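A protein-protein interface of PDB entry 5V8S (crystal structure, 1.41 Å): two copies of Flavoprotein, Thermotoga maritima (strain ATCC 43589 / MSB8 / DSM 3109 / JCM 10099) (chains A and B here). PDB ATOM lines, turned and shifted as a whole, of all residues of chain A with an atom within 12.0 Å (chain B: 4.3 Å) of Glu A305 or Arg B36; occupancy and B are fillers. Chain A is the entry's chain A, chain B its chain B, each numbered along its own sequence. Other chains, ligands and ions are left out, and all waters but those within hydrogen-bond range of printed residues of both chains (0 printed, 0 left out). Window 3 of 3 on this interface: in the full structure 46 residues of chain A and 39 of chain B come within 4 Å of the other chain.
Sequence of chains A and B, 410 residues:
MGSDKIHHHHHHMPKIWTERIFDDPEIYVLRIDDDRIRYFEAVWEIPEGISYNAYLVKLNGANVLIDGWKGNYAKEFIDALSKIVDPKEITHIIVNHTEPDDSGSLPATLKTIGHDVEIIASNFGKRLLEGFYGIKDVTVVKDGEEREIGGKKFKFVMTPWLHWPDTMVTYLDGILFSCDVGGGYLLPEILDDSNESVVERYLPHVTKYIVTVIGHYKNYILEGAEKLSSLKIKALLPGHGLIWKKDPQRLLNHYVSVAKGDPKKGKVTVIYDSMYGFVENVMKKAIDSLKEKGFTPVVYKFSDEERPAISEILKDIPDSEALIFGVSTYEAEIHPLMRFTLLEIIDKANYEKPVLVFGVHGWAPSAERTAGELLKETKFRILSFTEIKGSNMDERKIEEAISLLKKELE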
ATOM      1  N   TYR A 272     -21.952  -9.903 -16.609  1.00  0.00           N
ATOM      2  CA  TYR A 272     -22.986 -10.859 -16.977  1.00  0.00           C
ATOM      3  C   TYR A 272     -22.663 -12.266 -16.513  1.00  0.00           C
ATOM      4  O   TYR A 272     -21.509 -12.628 -16.275  1.00  0.00           O
ATOM      5  CB  TYR A 272     -23.245 -10.849 -18.487  1.00  0.00           C
ATOM      6  CG  TYR A 272     -22.116 -11.296 -19.390  1.00  0.00           C
ATOM      7  CD1 TYR A 272     -21.145 -10.395 -19.827  1.00  0.00           C
ATOM      8  CD2 TYR A 272     -22.081 -12.575 -19.922  1.00  0.00           C
ATOM      9  CE1 TYR A 272     -20.137 -10.791 -20.674  1.00  0.00           C
ATOM     10  CE2 TYR A 272     -21.072 -12.971 -20.781  1.00  0.00           C
ATOM     11  CZ  TYR A 272     -20.115 -12.070 -21.182  1.00  0.00           C
ATOM     12  OH  TYR A 272     -19.113 -12.443 -22.070  1.00  0.00           O
ATOM     13  N   ASP A 273     -23.723 -13.070 -16.410  1.00  0.00           N
ATOM     14  CA  ASP A 273     -23.612 -14.502 -16.159  1.00  0.00           C
ATOM     15  C   ASP A 273     -24.209 -15.265 -17.333  1.00  0.00           C
ATOM     16  O   ASP A 273     -25.339 -14.989 -17.752  1.00  0.00           O
ATOM     17  CB  ASP A 273     -24.207 -14.941 -14.792  1.00  0.00           C
ATOM     18  CG  ASP A 273     -25.704 -14.618 -14.609  1.00  0.00           C
ATOM     19  OD1 ASP A 273     -26.301 -13.867 -15.410  1.00  0.00           O
ATOM     20  OD2 ASP A 273     -26.282 -15.146 -13.604  1.00  0.00           O
ATOM     21  N   SER A 274     -23.443 -16.221 -17.862  1.00  0.00           N
ATOM     22  CA  SER A 274     -23.843 -16.983 -19.032  1.00  0.00           C
ATOM     23  C   SER A 274     -23.839 -18.428 -18.568  1.00  0.00           C
ATOM     24  O   SER A 274     -22.769 -19.045 -18.465  1.00  0.00           O
ATOM     25  CB  SER A 274     -22.888 -16.710 -20.181  1.00  0.00           C
ATOM     26  OG  SER A 274     -23.286 -17.422 -21.326  1.00  0.00           O
ATOM     27  N   MET A 275     -25.043 -18.927 -18.225  1.00  0.00           N
ATOM     28  CA  MET A 275     -25.206 -20.282 -17.712  1.00  0.00           C
ATOM     29  C   MET A 275     -24.924 -21.306 -18.788  1.00  0.00           C
ATOM     30  O   MET A 275     -24.382 -22.369 -18.481  1.00  0.00           O
ATOM     31  CB  MET A 275     -26.626 -20.483 -17.167  1.00  0.00           C
ATOM     32  CG  MET A 275     -26.881 -19.841 -15.785  1.00  0.00           C
ATOM     33  SD  MET A 275     -28.611 -19.862 -15.163  1.00  0.00           S
ATOM     34  CE  MET A 275     -28.820 -21.612 -14.864  1.00  0.00           C
ATOM     35  N   TYR A 276     -25.269 -20.998 -20.057  1.00  0.00           N
ATOM     36  CA  TYR A 276     -25.124 -21.945 -21.158  1.00  0.00           C
ATOM     37  C   TYR A 276     -24.505 -21.391 -22.427  1.00  0.00           C
ATOM     38  O   TYR A 276     -24.245 -22.187 -23.329  1.00  0.00           O
ATOM     39  CB  TYR A 276     -26.475 -22.566 -21.580  1.00  0.00           C
ATOM     40  CG  TYR A 276     -27.391 -22.945 -20.434  1.00  0.00           C
ATOM     41  CD1 TYR A 276     -27.070 -23.984 -19.573  1.00  0.00           C
ATOM     42  CD2 TYR A 276     -28.584 -22.269 -20.226  1.00  0.00           C
ATOM     43  CE1 TYR A 276     -27.876 -24.301 -18.514  1.00  0.00           C
ATOM     44  CE2 TYR A 276     -29.412 -22.583 -19.174  1.00  0.00           C
ATOM     45  CZ  TYR A 276     -29.053 -23.599 -18.317  1.00  0.00           C
ATOM     46  OH  TYR A 276     -29.883 -23.899 -17.275  1.00  0.00           O
ATOM     47  N   GLY A 277     -24.311 -20.081 -22.569  1.00  0.00           N
ATOM     48  CA  GLY A 277     -23.780 -19.502 -23.798  1.00  0.00           C
ATOM     49  C   GLY A 277     -24.727 -18.579 -24.548  1.00  0.00           C
ATOM     50  O   GLY A 277     -24.267 -17.772 -25.376  1.00  0.00           O
ATOM     51  N   GLU A 280     -23.887 -15.036 -23.338  1.00  0.00           N
ATOM     52  CA  GLU A 280     -22.604 -14.655 -23.922  1.00  0.00           C
ATOM     53  C   GLU A 280     -22.755 -14.221 -25.379  1.00  0.00           C
ATOM     54  O   GLU A 280     -22.107 -13.263 -25.817  1.00  0.00           O
ATOM     55  CB  GLU A 280     -21.634 -15.832 -23.803  1.00  0.00           C
ATOM     56  CG  GLU A 280     -20.443 -15.806 -24.762  1.00  0.00           C
ATOM     57  CD  GLU A 280     -19.391 -14.854 -24.310  1.00  0.00           C
ATOM     58  OE1 GLU A 280     -19.399 -14.545 -23.108  1.00  0.00           O
ATOM     59  OE2 GLU A 280     -18.575 -14.397 -25.151  1.00  0.00           O
ATOM     60  N   TYR A 300     -16.736  -8.353 -17.270  1.00  0.00           N
ATOM     61  CA  TYR A 300     -16.691  -9.363 -16.220  1.00  0.00           C
ATOM     62  C   TYR A 300     -17.740 -10.424 -16.518  1.00  0.00           C
ATOM     63  O   TYR A 300     -18.936 -10.124 -16.526  1.00  0.00           O
ATOM     64  CB  TYR A 300     -16.947  -8.733 -14.854  1.00  0.00           C
ATOM     65  CG  TYR A 300     -15.807  -7.853 -14.433  1.00  0.00           C
ATOM     66  CD1 TYR A 300     -14.618  -8.414 -13.999  1.00  0.00           C
ATOM     67  CD2 TYR A 300     -15.906  -6.466 -14.484  1.00  0.00           C
ATOM     68  CE1 TYR A 300     -13.557  -7.621 -13.601  1.00  0.00           C
ATOM     69  CE2 TYR A 300     -14.833  -5.661 -14.108  1.00  0.00           C
ATOM     70  CZ  TYR A 300     -13.661  -6.242 -13.678  1.00  0.00           C
ATOM     71  OH  TYR A 300     -12.590  -5.449 -13.286  1.00  0.00           O
ATOM     72  N   LYS A 301     -17.295 -11.657 -16.726  1.00  0.00           N
ATOM     73  CA  LYS A 301     -18.166 -12.752 -17.129  1.00  0.00           C
ATOM     74  C   LYS A 301     -18.115 -13.884 -16.109  1.00  0.00           C
ATOM     75  O   LYS A 301     -17.038 -14.401 -15.809  1.00  0.00           O
ATOM     76  CB  LYS A 301     -17.722 -13.313 -18.495  1.00  0.00           C
ATOM     77  CG  LYS A 301     -18.518 -14.537 -18.964  1.00  0.00           C
ATOM     78  CD  LYS A 301     -17.764 -15.464 -19.953  1.00  0.00           C
ATOM     79  CE  LYS A 301     -16.819 -14.775 -20.875  1.00  0.00           C
ATOM     80  NZ  LYS A 301     -16.198 -15.781 -21.815  1.00  0.00           N
ATOM     81  N   PHE A 302     -19.285 -14.299 -15.620  1.00  0.00           N
ATOM     82  CA  PHE A 302     -19.430 -15.533 -14.841  1.00  0.00           C
ATOM     83  C   PHE A 302     -19.854 -16.638 -15.806  1.00  0.00           C
ATOM     84  O   PHE A 302     -20.953 -16.591 -16.349  1.00  0.00           O
ATOM     85  CB  PHE A 302     -20.520 -15.381 -13.789  1.00  0.00           C
ATOM     86  CG  PHE A 302     -20.210 -14.366 -12.713  1.00  0.00           C
ATOM     87  CD1 PHE A 302     -19.437 -14.708 -11.630  1.00  0.00           C
ATOM     88  CD2 PHE A 302     -20.707 -13.089 -12.792  1.00  0.00           C
ATOM     89  CE1 PHE A 302     -19.154 -13.780 -10.636  1.00  0.00           C
ATOM     90  CE2 PHE A 302     -20.421 -12.135 -11.794  1.00  0.00           C
ATOM     91  CZ  PHE A 302     -19.663 -12.498 -10.725  1.00  0.00           C
ATOM     92  N   SER A 303     -19.004 -17.626 -16.007  1.00  0.00           N
ATOM     93  CA  SER A 303     -19.325 -18.721 -16.912  1.00  0.00           C
ATOM     94  C   SER A 303     -19.033 -20.042 -16.219  1.00  0.00           C
ATOM     95  O   SER A 303     -18.647 -20.087 -15.042  1.00  0.00           O
ATOM     96  CB  SER A 303     -18.505 -18.641 -18.196  1.00  0.00           C
ATOM     97  OG  SER A 303     -17.149 -18.964 -17.928  1.00  0.00           O
ATOM     98  N   ASP A 304     -19.197 -21.126 -16.971  1.00  0.00           N
ATOM     99  CA  ASP A 304     -18.902 -22.430 -16.403  1.00  0.00           C
ATOM    100  C   ASP A 304     -17.402 -22.693 -16.283  1.00  0.00           C
ATOM    101  O   ASP A 304     -17.012 -23.709 -15.714  1.00  0.00           O
ATOM    102  CB  ASP A 304     -19.672 -23.535 -17.154  1.00  0.00           C
ATOM    103  CG  ASP A 304     -19.233 -23.729 -18.587  1.00  0.00           C
ATOM    104  OD1 ASP A 304     -18.133 -23.308 -18.966  1.00  0.00           O
ATOM    105  OD2 ASP A 304     -20.011 -24.324 -19.361  1.00  0.00           O
ATOM    106  N   GLU A 305     -16.550 -21.790 -16.760  1.00  0.00           N
ATOM    107  CA  GLU A 305     -15.116 -21.954 -16.609  1.00  0.00           C
ATOM    108  C   GLU A 305     -14.442 -20.795 -15.904  1.00  0.00           C
ATOM    109  O   GLU A 305     -13.298 -20.951 -15.465  1.00  0.00           O
ATOM    110  CB  GLU A 305     -14.435 -22.134 -17.976  1.00  0.00           C
ATOM    111  CG  GLU A 305     -14.680 -23.475 -18.592  1.00  0.00           C
ATOM    112  CD  GLU A 305     -13.717 -23.785 -19.717  1.00  0.00           C
ATOM    113  OE1 GLU A 305     -12.597 -23.233 -19.740  1.00  0.00           O
ATOM    114  OE2 GLU A 305     -14.086 -24.586 -20.582  1.00  0.00           O
ATOM    115  N   GLU A 306     -15.103 -19.652 -15.770  1.00  0.00           N
ATOM    116  CA  GLU A 306     -14.436 -18.486 -15.210  1.00  0.00           C
ATOM    117  C   GLU A 306     -15.344 -17.728 -14.257  1.00  0.00           C
ATOM    118  O   GLU A 306     -16.563 -17.702 -14.395  1.00  0.00           O
ATOM    119  CB  GLU A 306     -13.803 -17.563 -16.278  1.00  0.00           C
ATOM    120  CG  GLU A 306     -14.674 -17.147 -17.456  1.00  0.00           C
ATOM    121  CD  GLU A 306     -13.855 -16.459 -18.575  1.00  0.00           C
ATOM    122  OE1 GLU A 306     -12.635 -16.720 -18.691  1.00  0.00           O
ATOM    123  OE2 GLU A 306     -14.429 -15.651 -19.338  1.00  0.00           O
ATOM    124  N   ARG A 307     -14.708 -17.072 -13.312  1.00  0.00           N
ATOM    125  CA  ARG A 307     -15.362 -16.467 -12.161  1.00  0.00           C
ATOM    126  C   ARG A 307     -14.545 -15.232 -11.789  1.00  0.00           C
ATOM    127  O   ARG A 307     -13.433 -15.375 -11.272  1.00  0.00           O
ATOM    128  CB  ARG A 307     -15.348 -17.511 -11.042  1.00  0.00           C
ATOM    129  CG  ARG A 307     -15.704 -17.070  -9.651  1.00  0.00           C
ATOM    130  CD  ARG A 307     -17.171 -16.957  -9.434  1.00  0.00           C
ATOM    131  NE  ARG A 307     -17.930 -18.125  -9.888  1.00  0.00           N
ATOM    132  CZ  ARG A 307     -18.235 -19.183  -9.140  1.00  0.00           C
ATOM    133  NH1 ARG A 307     -17.856 -19.272  -7.865  1.00  0.00           N
ATOM    134  NH2 ARG A 307     -18.974 -20.132  -9.670  1.00  0.00           N
ATOM    135  N   PRO A 308     -15.034 -14.022 -12.042  1.00  0.00           N
ATOM    136  CA  PRO A 308     -14.304 -12.826 -11.607  1.00  0.00           C
ATOM    137  C   PRO A 308     -14.330 -12.656 -10.104  1.00  0.00           C
ATOM    138  O   PRO A 308     -15.203 -13.157  -9.401  1.00  0.00           O
ATOM    139  CB  PRO A 308     -15.065 -11.676 -12.269  1.00  0.00           C
ATOM    140  CG  PRO A 308     -16.373 -12.222 -12.608  1.00  0.00           C
ATOM    141  CD  PRO A 308     -16.196 -13.667 -12.864  1.00  0.00           C
ATOM    142  N   ALA A 309     -13.363 -11.893  -9.631  1.00  0.00           N
ATOM    143  CA  ALA A 309     -13.342 -11.448  -8.247  1.00  0.00           C
ATOM    144  C   ALA A 309     -14.312 -10.292  -8.059  1.00  0.00           C
ATOM    145  O   ALA A 309     -14.273  -9.314  -8.800  1.00  0.00           O
ATOM    146  CB  ALA A 309     -11.935 -10.993  -7.865  1.00  0.00           C
ATOM    147  N   LEU A 337     -24.632 -15.868  -8.275  1.00  0.00           N
ATOM    148  CA  LEU A 337     -23.481 -14.981  -8.393  1.00  0.00           C
ATOM    149  C   LEU A 337     -23.896 -13.584  -8.830  1.00  0.00           C
ATOM    150  O   LEU A 337     -23.349 -12.592  -8.341  1.00  0.00           O
ATOM    151  CB  LEU A 337     -22.441 -15.563  -9.340  1.00  0.00           C
ATOM    152  CG  LEU A 337     -21.631 -16.691  -8.716  1.00  0.00           C
ATOM    153  CD1 LEU A 337     -21.054 -17.610  -9.735  1.00  0.00           C
ATOM    154  CD2 LEU A 337     -20.504 -16.059  -7.905  1.00  0.00           C
ATOM    155  N   MET B  13      -7.255 -34.446 -24.356  1.00  0.00           N
ATOM    156  CA  MET B  13      -8.606 -34.444 -24.900  1.00  0.00           C
ATOM    157  C   MET B  13      -9.559 -35.141 -23.930  1.00  0.00           C
ATOM    158  O   MET B  13      -9.139 -36.035 -23.196  1.00  0.00           O
ATOM    159  CB  MET B  13      -8.623 -35.200 -26.235  1.00  0.00           C
ATOM    160  CG  MET B  13      -7.834 -34.510 -27.343  1.00  0.00           C
ATOM    161  SD  MET B  13      -8.492 -32.876 -27.749  1.00  0.00           S
ATOM    162  CE  MET B  13     -10.188 -33.257 -28.187  1.00  0.00           C
ATOM    163  N   PRO B  14     -10.833 -34.746 -23.868  1.00  0.00           N
ATOM    164  CA  PRO B  14     -11.751 -35.420 -22.934  1.00  0.00           C
ATOM    165  C   PRO B  14     -11.892 -36.895 -23.271  1.00  0.00           C
ATOM    166  O   PRO B  14     -11.955 -37.280 -24.436  1.00  0.00           O
ATOM    167  CB  PRO B  14     -13.078 -34.678 -23.129  1.00  0.00           C
ATOM    168  CG  PRO B  14     -12.712 -33.387 -23.822  1.00  0.00           C
ATOM    169  CD  PRO B  14     -11.536 -33.739 -24.678  1.00  0.00           C
ATOM    170  N   ASP B  34     -16.395 -34.527 -18.942  1.00  0.00           N
ATOM    171  CA  ASP B  34     -16.064 -33.099 -18.999  1.00  0.00           C
ATOM    172  C   ASP B  34     -15.146 -32.760 -17.829  1.00  0.00           C
ATOM    173  O   ASP B  34     -15.602 -32.514 -16.714  1.00  0.00           O
ATOM    174  CB  ASP B  34     -17.321 -32.237 -18.993  1.00  0.00           C
ATOM    175  CG  ASP B  34     -17.024 -30.777 -19.310  1.00  0.00           C
ATOM    176  OD1 ASP B  34     -15.840 -30.419 -19.424  1.00  0.00           O
ATOM    177  OD2 ASP B  34     -17.989 -29.996 -19.446  1.00  0.00           O
ATOM    178  N   ASP B  35     -13.842 -32.728 -18.102  1.00  0.00           N
ATOM    179  CA  ASP B  35     -12.836 -32.309 -17.143  1.00  0.00           C
ATOM    180  C   ASP B  35     -12.383 -30.875 -17.383  1.00  0.00           C
ATOM    181  O   ASP B  35     -11.405 -30.438 -16.767  1.00  0.00           O
ATOM    182  CB  ASP B  35     -11.638 -33.263 -17.195  1.00  0.00           C
ATOM    183  CG  ASP B  35     -11.034 -33.373 -18.582  1.00  0.00           C
ATOM    184  OD1 ASP B  35     -11.399 -32.595 -19.488  1.00  0.00           O
ATOM    185  OD2 ASP B  35     -10.179 -34.262 -18.786  1.00  0.00           O
ATOM    186  N   ARG B  36     -13.073 -30.137 -18.260  1.00  0.00           N
ATOM    187  CA  ARG B  36     -12.794 -28.722 -18.504  1.00  0.00           C
ATOM    188  C   ARG B  36     -13.670 -27.797 -17.669  1.00  0.00           C
ATOM    189  O   ARG B  36     -13.200 -26.764 -17.183  1.00  0.00           O
ATOM    190  CB  ARG B  36     -13.013 -28.390 -19.988  1.00  0.00           C
ATOM    191  CG  ARG B  36     -12.089 -29.101 -20.964  1.00  0.00           C
ATOM    192  CD  ARG B  36     -12.290 -28.568 -22.384  1.00  0.00           C
ATOM    193  NE  ARG B  36     -11.626 -29.416 -23.368  1.00  0.00           N
ATOM    194  CZ  ARG B  36     -11.855 -29.381 -24.679  1.00  0.00           C
ATOM    195  NH1 ARG B  36     -12.742 -28.533 -25.195  1.00  0.00           N
ATOM    196  NH2 ARG B  36     -11.192 -30.203 -25.480  1.00  0.00           N
ATOM    197  N   ILE B  37     -14.938 -28.150 -17.493  1.00  0.00           N
ATOM    198  CA  ILE B  37     -15.860 -27.345 -16.712  1.00  0.00           C
ATOM    199  C   ILE B  37     -15.361 -27.209 -15.281  1.00  0.00           C
ATOM    200  O   ILE B  37     -14.761 -28.129 -14.717  1.00  0.00           O
ATOM    201  CB  ILE B  37     -17.251 -28.002 -16.771  1.00  0.00           C
ATOM    202  CG1 ILE B  37     -18.321 -27.084 -16.201  1.00  0.00           C
ATOM    203  CG2 ILE B  37     -17.275 -29.410 -16.109  1.00  0.00           C
ATOM    204  CD1 ILE B  37     -19.718 -27.473 -16.572  1.00  0.00           C
ATOM    205  N   ARG B  38     -15.596 -26.046 -14.697  1.00  0.00           N
ATOM    206  CA  ARG B  38     -15.260 -25.768 -13.309  1.00  0.00           C
ATOM    207  C   ARG B  38     -16.480 -25.485 -12.451  1.00  0.00           C
ATOM    208  O   ARG B  38     -16.475 -25.816 -11.266  1.00  0.00           O
ATOM    209  CB  ARG B  38     -14.301 -24.559 -13.223  1.00  0.00           C
ATOM    210  CG  ARG B  38     -12.943 -24.821 -13.881  1.00  0.00           C
ATOM    211  CD  ARG B  38     -12.000 -23.592 -13.732  1.00  0.00           C
ATOM    212  NE  ARG B  38     -11.943 -23.101 -12.357  1.00  0.00           N
ATOM    213  CZ  ARG B  38     -11.226 -23.659 -11.383  1.00  0.00           C
ATOM    214  NH1 ARG B  38     -10.494 -24.742 -11.621  1.00  0.00           N
ATOM    215  NH2 ARG B  38     -11.245 -23.141 -10.160  1.00  0.00           N
ATOM    216  N   TYR B  39     -17.511 -24.868 -13.020  1.00  0.00           N
ATOM    217  CA  TYR B  39     -18.677 -24.384 -12.287  1.00  0.00           C
ATOM    218  C   TYR B  39     -19.925 -24.836 -13.038  1.00  0.00           C
ATOM    219  O   TYR B  39     -20.238 -24.302 -14.110  1.00  0.00           O
ATOM    220  CB  TYR B  39     -18.641 -22.852 -12.179  1.00  0.00           C
ATOM    221  CG  TYR B  39     -17.340 -22.330 -11.631  1.00  0.00           C
ATOM    222  CD1 TYR B  39     -16.974 -22.571 -10.312  1.00  0.00           C
ATOM    223  CD2 TYR B  39     -16.479 -21.578 -12.423  1.00  0.00           C
ATOM    224  CE1 TYR B  39     -15.769 -22.081  -9.810  1.00  0.00           C
ATOM    225  CE2 TYR B  39     -15.275 -21.100 -11.932  1.00  0.00           C
ATOM    226  CZ  TYR B  39     -14.927 -21.350 -10.630  1.00  0.00           C
ATOM    227  OH  TYR B  39     -13.736 -20.862 -10.141  1.00  0.00           O
ATOM    228  N   TYR B  73     -18.884 -29.619 -27.150  1.00  0.00           N
ATOM    229  CA  TYR B  73     -18.416 -30.935 -27.562  1.00  0.00           C
ATOM    230  C   TYR B  73     -19.217 -31.485 -28.743  1.00  0.00           C
ATOM    231  O   TYR B  73     -19.218 -32.703 -28.994  1.00  0.00           O
ATOM    232  CB  TYR B  73     -18.453 -31.897 -26.369  1.00  0.00           C
ATOM    233  CG  TYR B  73     -17.553 -31.483 -25.216  1.00  0.00           C
ATOM    234  CD1 TYR B  73     -16.181 -31.357 -25.406  1.00  0.00           C
ATOM    235  CD2 TYR B  73     -18.065 -31.233 -23.952  1.00  0.00           C
ATOM    236  CE1 TYR B  73     -15.344 -30.989 -24.376  1.00  0.00           C
ATOM    237  CE2 TYR B  73     -17.224 -30.865 -22.910  1.00  0.00           C
ATOM    238  CZ  TYR B  73     -15.871 -30.757 -23.129  1.00  0.00           C
ATOM    239  OH  TYR B  73     -15.020 -30.399 -22.115  1.00  0.00           O
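No position is printed for both chains.
OG of Ser A303 lies close to N of Glu A305.
The side-chain hydroxyl of Ser A303 is in hydrogen-bond range of the backbone NH of Glu A306 (3.1 Å).
OD1 of Asp B34 sits at hydrogen-bond distance from N of Arg B36 (3.0 Å).
The side-chain carboxylate (OD1) of Asp B34 lies within hydrogen-bond range of the backbone NH (N) of Ile B37, at 3.1 Å.
NH2 of Arg B38 sits at hydrogen-bond distance from OH of Tyr B39.
Printed residues of chain B that touch a printed residue of chain A: Arg B36, Ile B37, Arg B38 and Tyr B39.
Among the printed residues, no Asp or Glu carboxylate lies within 4 Å of a Lys or Arg side-chain nitrogen of the other chain.
N of Arg B38 is in hydrogen-bond range of O of Asp A304.
O of Asp A304 is in hydrogen-bond range of N of Tyr B39 (3.0 Å).
Of the printed residues of chain B, Glu A305 touches Arg B36 and Arg B38.
Arg B36 touches just one residue of chain A: Glu A305 (3.9 Å).
No residue of chain A comes within 4 Å of Pro B14.
No residue of chain A comes within 4 Å of Asp B35.
Ile B37 touches just one residue of chain A: Asp A304.
Arg B38 touches two residues of chain A.
Printed residues of chain B within 4 Å of Arg A307: Tyr B39 (3.2 Å).
Of the printed residues of chain B, Ser A303 touches Tyr B39 (3.7 Å).
Printed residues of chain B within 4 Å of Asp A304: Ile B37 (3.7 Å), Arg B38 (2.9 Å) and Tyr B39 (3.0 Å).
Ala A309 touches none of the printed residues of chain B.
Glu A280 touches none of the printed residues of chain B.
The nearest residue of chain B that does not touch Glu A305 is Tyr B39 (4.1 Å).
The nearest residue of chain A that does not touch Arg B36 is Asp A304 (5.1 Å).
The nearest printed residue of chain B that does not touch Asp A304 is Arg B36 (5.1 Å).
Among the printed residues, pairs that only touch across the chains: Ser A303 with Tyr B39 (3.7 Å), Asp A304 with Ile B37 (3.7 Å), Glu A305 with Arg B36 (3.9 Å), Glu A305 with Arg B38 (3.4 Å) and Arg A307 with Tyr B39 (3.2 Å).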
